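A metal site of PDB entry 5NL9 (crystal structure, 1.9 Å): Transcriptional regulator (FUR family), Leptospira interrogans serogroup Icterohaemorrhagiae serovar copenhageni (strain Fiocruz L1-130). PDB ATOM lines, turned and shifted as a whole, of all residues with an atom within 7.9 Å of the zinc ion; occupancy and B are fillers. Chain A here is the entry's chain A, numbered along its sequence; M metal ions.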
ATOM      1  N   PRO A  40     -24.834 -13.122  16.636  1.00  0.00           N
ATOM      2  CA  PRO A  40     -23.736 -12.138  16.659  1.00  0.00           C
ATOM      3  C   PRO A  40     -24.155 -10.897  15.884  1.00  0.00           C
ATOM      4  O   PRO A  40     -24.621 -10.981  14.746  1.00  0.00           O
ATOM      5  CB  PRO A  40     -22.586 -12.880  15.946  1.00  0.00           C
ATOM      6  CG  PRO A  40     -23.005 -14.336  15.917  1.00  0.00           C
ATOM      7  CD  PRO A  40     -24.499 -14.279  15.786  1.00  0.00           C
ATOM      8  N   GLN A  41     -24.120  -9.752  16.554  1.00  0.00           N
ATOM      9  CA  GLN A  41     -24.523  -8.488  15.943  1.00  0.00           C
ATOM     10  C   GLN A  41     -23.791  -7.343  16.636  1.00  0.00           C
ATOM     11  O   GLN A  41     -23.247  -7.535  17.725  1.00  0.00           O
ATOM     12  CB  GLN A  41     -26.061  -8.305  16.014  1.00  0.00           C
ATOM     13  CG  GLN A  41     -26.663  -8.358  17.431  1.00  0.00           C
ATOM     14  CD  GLN A  41     -28.165  -8.590  17.407  1.00  0.00           C
ATOM     15  OE1 GLN A  41     -28.883  -8.189  16.499  1.00  0.00           O
ATOM     16  NE2 GLN A  41     -28.702  -9.225  18.440  1.00  0.00           N
ATOM     17  N   HIS A  42     -23.753  -6.176  16.013  1.00  0.00           N
ATOM     18  CA  HIS A  42     -23.072  -4.943  16.468  1.00  0.00           C
ATOM     19  C   HIS A  42     -24.071  -3.822  16.279  1.00  0.00           C
ATOM     20  O   HIS A  42     -24.272  -3.387  15.149  1.00  0.00           O
ATOM     21  CB  HIS A  42     -21.846  -4.651  15.568  1.00  0.00           C
ATOM     22  CG  HIS A  42     -20.880  -5.794  15.515  1.00  0.00           C
ATOM     23  ND1 HIS A  42     -20.949  -6.751  14.512  1.00  0.00           N
ATOM     24  CD2 HIS A  42     -19.831  -6.069  16.315  1.00  0.00           C
ATOM     25  CE1 HIS A  42     -19.993  -7.628  14.781  1.00  0.00           C
ATOM     26  NE2 HIS A  42     -19.270  -7.255  15.842  1.00  0.00           N
ATOM     27  N   ASN A  78     -20.111  -6.397  24.543  1.00  0.00           N
ATOM     28  CA  ASN A  78     -18.864  -5.600  24.625  1.00  0.00           C
ATOM     29  C   ASN A  78     -18.965  -4.306  23.813  1.00  0.00           C
ATOM     30  O   ASN A  78     -19.578  -4.290  22.754  1.00  0.00           O
ATOM     31  CB  ASN A  78     -17.639  -6.405  24.206  1.00  0.00           C
ATOM     32  CG  ASN A  78     -17.076  -7.274  25.311  1.00  0.00           C
ATOM     33  OD1 ASN A  78     -17.408  -7.136  26.490  1.00  0.00           O
ATOM     34  ND2 ASN A  78     -16.179  -8.170  24.955  1.00  0.00           N
ATOM     35  N   LEU A  80     -17.769  -1.540  21.339  1.00  0.00           N
ATOM     36  CA  LEU A  80     -16.919  -1.483  20.143  1.00  0.00           C
ATOM     37  C   LEU A  80     -17.050  -0.089  19.518  1.00  0.00           C
ATOM     38  O   LEU A  80     -18.126   0.274  19.053  1.00  0.00           O
ATOM     39  CB  LEU A  80     -17.325  -2.579  19.123  1.00  0.00           C
ATOM     40  CG  LEU A  80     -16.537  -2.596  17.803  1.00  0.00           C
ATOM     41  CD1 LEU A  80     -15.143  -3.174  18.007  1.00  0.00           C
ATOM     42  CD2 LEU A  80     -17.278  -3.369  16.730  1.00  0.00           C
ATOM     43  N   TYR A  89     -22.556  -1.929  20.277  1.00  0.00           N
ATOM     44  CA  TYR A  89     -22.696  -2.935  21.322  1.00  0.00           C
ATOM     45  C   TYR A  89     -22.627  -4.251  20.600  1.00  0.00           C
ATOM     46  O   TYR A  89     -23.470  -4.537  19.736  1.00  0.00           O
ATOM     47  CB  TYR A  89     -24.048  -2.723  22.037  1.00  0.00           C
ATOM     48  CG  TYR A  89     -24.040  -1.416  22.806  1.00  0.00           C
ATOM     49  CD1 TYR A  89     -24.420  -0.217  22.189  1.00  0.00           C
ATOM     50  CD2 TYR A  89     -23.572  -1.356  24.114  1.00  0.00           C
ATOM     51  CE1 TYR A  89     -24.367   1.008  22.871  1.00  0.00           C
ATOM     52  CE2 TYR A  89     -23.529  -0.147  24.811  1.00  0.00           C
ATOM     53  CZ  TYR A  89     -23.909   1.032  24.173  1.00  0.00           C
ATOM     54  OH  TYR A  89     -23.846   2.228  24.853  1.00  0.00           O
ATOM     55  N   ASP A  90     -21.591  -5.020  20.923  1.00  0.00           N
ATOM     56  CA  ASP A  90     -21.272  -6.285  20.261  1.00  0.00           C
ATOM     57  C   ASP A  90     -21.728  -7.471  21.114  1.00  0.00           C
ATOM     58  O   ASP A  90     -21.358  -7.561  22.270  1.00  0.00           O
ATOM     59  CB  ASP A  90     -19.741  -6.317  20.018  1.00  0.00           C
ATOM     60  CG  ASP A  90     -19.171  -7.419  19.127  1.00  0.00           C
ATOM     61  OD1 ASP A  90     -19.881  -8.415  18.876  1.00  0.00           O
ATOM     62  OD2 ASP A  90     -18.043  -7.215  18.582  1.00  0.00           O
ATOM     63  N   SER A  91     -22.529  -8.385  20.543  1.00  0.00           N
ATOM     64  CA  SER A  91     -23.046  -9.532  21.299  1.00  0.00           C
ATOM     65  C   SER A  91     -22.061 -10.702  21.272  1.00  0.00           C
ATOM     66  O   SER A  91     -22.336 -11.728  21.888  1.00  0.00           O
ATOM     67  CB  SER A  91     -24.413  -9.949  20.791  1.00  0.00           C
ATOM     68  OG  SER A  91     -24.261 -10.470  19.485  1.00  0.00           O
ATOM     69  N   ASN A  92     -20.910 -10.544  20.615  1.00  0.00           N
ATOM     70  CA  ASN A  92     -19.932 -11.628  20.661  1.00  0.00           C
ATOM     71  C   ASN A  92     -18.895 -11.139  21.684  1.00  0.00           C
ATOM     72  O   ASN A  92     -18.265 -10.098  21.474  1.00  0.00           O
ATOM     73  CB  ASN A  92     -19.324 -11.894  19.263  1.00  0.00           C
ATOM     74  CG  ASN A  92     -18.235 -12.928  19.196  1.00  0.00           C
ATOM     75  OD1 ASN A  92     -17.942 -13.655  20.145  1.00  0.00           O
ATOM     76  ND2 ASN A  92     -17.609 -13.018  18.040  1.00  0.00           N
ATOM     77  N   VAL A  93     -18.811 -11.831  22.842  1.00  0.00           N
ATOM     78  CA  VAL A  93     -17.890 -11.431  23.918  1.00  0.00           C
ATOM     79  C   VAL A  93     -16.534 -12.168  23.844  1.00  0.00           C
ATOM     80  O   VAL A  93     -15.622 -11.803  24.575  1.00  0.00           O
ATOM     81  CB  VAL A  93     -18.511 -11.513  25.343  1.00  0.00           C
ATOM     82  CG1 VAL A  93     -19.592 -10.444  25.533  1.00  0.00           C
ATOM     83  CG2 VAL A  93     -19.066 -12.907  25.634  1.00  0.00           C
ATOM     84  N   ILE A  94     -16.419 -13.190  23.001  1.00  0.00           N
ATOM     85  CA  ILE A  94     -15.177 -13.940  22.850  1.00  0.00           C
ATOM     86  C   ILE A  94     -14.233 -13.020  22.028  1.00  0.00           C
ATOM     87  O   ILE A  94     -14.705 -12.369  21.100  1.00  0.00           O
ATOM     88  CB  ILE A  94     -15.449 -15.305  22.163  1.00  0.00           C
ATOM     89  CG1 ILE A  94     -16.194 -16.253  23.130  1.00  0.00           C
ATOM     90  CG2 ILE A  94     -14.145 -15.956  21.628  1.00  0.00           C
ATOM     91  CD1 ILE A  94     -16.751 -17.513  22.517  1.00  0.00           C
ATOM     92  N   HIS A  95     -12.950 -12.918  22.406  1.00  0.00           N
ATOM     93  CA  HIS A  95     -11.991 -12.049  21.728  1.00  0.00           C
ATOM     94  C   HIS A  95     -11.986 -12.273  20.209  1.00  0.00           C
ATOM     95  O   HIS A  95     -11.834 -13.403  19.760  1.00  0.00           O
ATOM     96  CB  HIS A  95     -10.569 -12.204  22.311  1.00  0.00           C
ATOM     97  CG  HIS A  95      -9.528 -11.379  21.627  1.00  0.00           C
ATOM     98  ND1 HIS A  95      -9.467 -10.000  21.804  1.00  0.00           N
ATOM     99  CD2 HIS A  95      -8.545 -11.753  20.780  1.00  0.00           C
ATOM    100  CE1 HIS A  95      -8.449  -9.582  21.057  1.00  0.00           C
ATOM    101  NE2 HIS A  95      -7.866 -10.606  20.413  1.00  0.00           N
ATOM    102  N   HIS A  96     -12.220 -11.201  19.451  1.00  0.00           N
ATOM    103  CA  HIS A  96     -12.212 -11.281  18.000  1.00  0.00           C
ATOM    104  C   HIS A  96     -11.896  -9.918  17.359  1.00  0.00           C
ATOM    105  O   HIS A  96     -11.871  -8.897  18.058  1.00  0.00           O
ATOM    106  CB  HIS A  96     -13.547 -11.844  17.454  1.00  0.00           C
ATOM    107  CG  HIS A  96     -14.727 -10.957  17.738  1.00  0.00           C
ATOM    108  ND1 HIS A  96     -15.390 -10.991  18.942  1.00  0.00           N
ATOM    109  CD2 HIS A  96     -15.305 -10.016  16.954  1.00  0.00           C
ATOM    110  CE1 HIS A  96     -16.352 -10.079  18.853  1.00  0.00           C
ATOM    111  NE2 HIS A  96     -16.360  -9.495  17.662  1.00  0.00           N
ATOM    112  N   HIS A  97     -11.640  -9.901  16.042  1.00  0.00           N
ATOM    113  CA  HIS A  97     -11.372  -8.675  15.305  1.00  0.00           C
ATOM    114  C   HIS A  97     -12.501  -8.413  14.332  1.00  0.00           C
ATOM    115  O   HIS A  97     -13.494  -9.151  14.361  1.00  0.00           O
ATOM    116  CB  HIS A  97     -10.009  -8.776  14.583  1.00  0.00           C
ATOM    117  CG  HIS A  97      -8.911  -9.112  15.548  1.00  0.00           C
ATOM    118  ND1 HIS A  97      -8.573  -8.244  16.578  1.00  0.00           N
ATOM    119  CD2 HIS A  97      -8.211 -10.261  15.693  1.00  0.00           C
ATOM    120  CE1 HIS A  97      -7.632  -8.867  17.268  1.00  0.00           C
ATOM    121  NE2 HIS A  97      -7.370 -10.070  16.762  1.00  0.00           N
ATOM    122  N   HIS A  98     -12.391  -7.375  13.519  1.00  0.00           N
ATOM    123  CA  HIS A  98     -13.463  -6.980  12.596  1.00  0.00           C
ATOM    124  C   HIS A  98     -13.009  -6.567  11.219  1.00  0.00           C
ATOM    125  O   HIS A  98     -12.024  -5.863  11.066  1.00  0.00           O
ATOM    126  CB  HIS A  98     -14.218  -5.767  13.188  1.00  0.00           C
ATOM    127  CG  HIS A  98     -14.920  -6.077  14.457  1.00  0.00           C
ATOM    128  ND1 HIS A  98     -14.279  -5.928  15.681  1.00  0.00           N
ATOM    129  CD2 HIS A  98     -16.109  -6.676  14.656  1.00  0.00           C
ATOM    130  CE1 HIS A  98     -15.137  -6.377  16.586  1.00  0.00           C
ATOM    131  NE2 HIS A  98     -16.254  -6.828  16.013  1.00  0.00           N
ATOM    132  N   ALA A  99     -13.798  -6.970  10.224  1.00  0.00           N
ATOM    133  CA  ALA A  99     -13.629  -6.530   8.838  1.00  0.00           C
ATOM    134  C   ALA A  99     -14.864  -5.678   8.581  1.00  0.00           C
ATOM    135  O   ALA A  99     -15.984  -6.027   8.991  1.00  0.00           O
ATOM    136  CB  ALA A  99     -13.585  -7.719   7.898  1.00  0.00           C
ATOM    137  N   ILE A 107     -20.322  -4.829   9.224  1.00  0.00           N
ATOM    138  CA  ILE A 107     -19.231  -5.326  10.059  1.00  0.00           C
ATOM    139  C   ILE A 107     -19.288  -6.836  10.160  1.00  0.00           C
ATOM    140  O   ILE A 107     -20.347  -7.397  10.450  1.00  0.00           O
ATOM    141  CB  ILE A 107     -19.275  -4.615  11.459  1.00  0.00           C
ATOM    142  CG1 ILE A 107     -19.197  -3.106  11.319  1.00  0.00           C
ATOM    143  CG2 ILE A 107     -18.235  -5.156  12.451  1.00  0.00           C
ATOM    144  CD1 ILE A 107     -20.018  -2.393  12.352  1.00  0.00           C
ATOM    145  N   TYR A 108     -18.124  -7.471   9.979  1.00  0.00           N
ATOM    146  CA  TYR A 108     -17.971  -8.904  10.058  1.00  0.00           C
ATOM    147  C   TYR A 108     -16.953  -9.250  11.168  1.00  0.00           C
ATOM    148  O   TYR A 108     -15.883  -8.672  11.213  1.00  0.00           O
ATOM    149  CB  TYR A 108     -17.474  -9.480   8.709  1.00  0.00           C
ATOM    150  CG  TYR A 108     -18.385  -9.144   7.542  1.00  0.00           C
ATOM    151  CD1 TYR A 108     -18.337  -7.901   6.934  1.00  0.00           C
ATOM    152  CD2 TYR A 108     -19.376 -10.034   7.130  1.00  0.00           C
ATOM    153  CE1 TYR A 108     -19.202  -7.561   5.899  1.00  0.00           C
ATOM    154  CE2 TYR A 108     -20.228  -9.719   6.070  1.00  0.00           C
ATOM    155  CZ  TYR A 108     -20.139  -8.471   5.458  1.00  0.00           C
ATOM    156  OH  TYR A 108     -20.988  -8.137   4.428  1.00  0.00           O
ATOM    157  N   ASP A 109     -17.299 -10.216  12.029  1.00  0.00           N
ATOM    158  CA  ASP A 109     -16.378 -10.716  13.050  1.00  0.00           C
ATOM    159  C   ASP A 109     -15.376 -11.616  12.320  1.00  0.00           C
ATOM    160  O   ASP A 109     -15.751 -12.360  11.415  1.00  0.00           O
ATOM    161  CB  ASP A 109     -17.152 -11.543  14.096  1.00  0.00           C
ATOM    162  CG  ASP A 109     -17.900 -10.705  15.090  1.00  0.00           C
ATOM    163  OD1 ASP A 109     -17.700  -9.463  15.096  1.00  0.00           O
ATOM    164  OD2 ASP A 109     -18.586 -11.282  15.960  1.00  0.00           O
ATOM    165  N   ILE A 110     -14.078 -11.461  12.638  1.00  0.00           N
ATOM    166  CA  ILE A 110     -13.016 -12.254  12.032  1.00  0.00           C
ATOM    167  C   ILE A 110     -11.974 -12.524  13.099  1.00  0.00           C
ATOM    168  O   ILE A 110     -11.850 -11.744  14.036  1.00  0.00           O
ATOM    169  CB  ILE A 110     -12.447 -11.585  10.744  1.00  0.00           C
ATOM    170  CG1 ILE A 110     -11.606 -12.543   9.913  1.00  0.00           C
ATOM    171  CG2 ILE A 110     -11.712 -10.252  11.018  1.00  0.00           C
ATOM    172  CD1 ILE A 110     -11.428 -12.053   8.480  1.00  0.00           C
HETATM  173 ZN    ZN M   1     -17.682  -8.140  16.794  1.00  0.00          ZN
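OD1 of Asp 90 sits at hydrogen-bond distance from N of Asn 92 (2.9 Å). A ring nitrogen (ND1) of His 96 is in hydrogen-bond range of the side-chain amide nitrogen of Asn 92. ND1 of His 96 lies within hydrogen-bond range of O of Ile 94, at 2.7 Å. OD2 of Asp 109 is in hydrogen-bond range of ND2 of Asn 92, at 2.9 Å. The backbone carbonyl oxygen (O) of Asn 78 is in hydrogen-bond range of the backbone NH (N) of Asp 90 (2.8 Å).
Five residues have an atom within 4 Å of the zinc ion: His 42, Asp 90, His 96, His 98 and Asp 109. Along chain A the residues within 4 Å of the zinc ion span positions 42 to 109. The nearest printed residue that does not touch the zinc ion is Asn 92 (4.8 Å).
The zinc ion is bound by OD2 of Asp 90 (2.0 Å). NE2 of His 42 binds the zinc ion, at 2.1 Å. NE2 of His 96 binds the zinc ion (2.1 Å). A ring nitrogen (NE2) of His 98 is bound to the zinc ion (2.1 Å). The zinc ion is bound by OD1 of Asp 109 (2.2 Å). The zinc ion has five donor atoms within binding distance.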
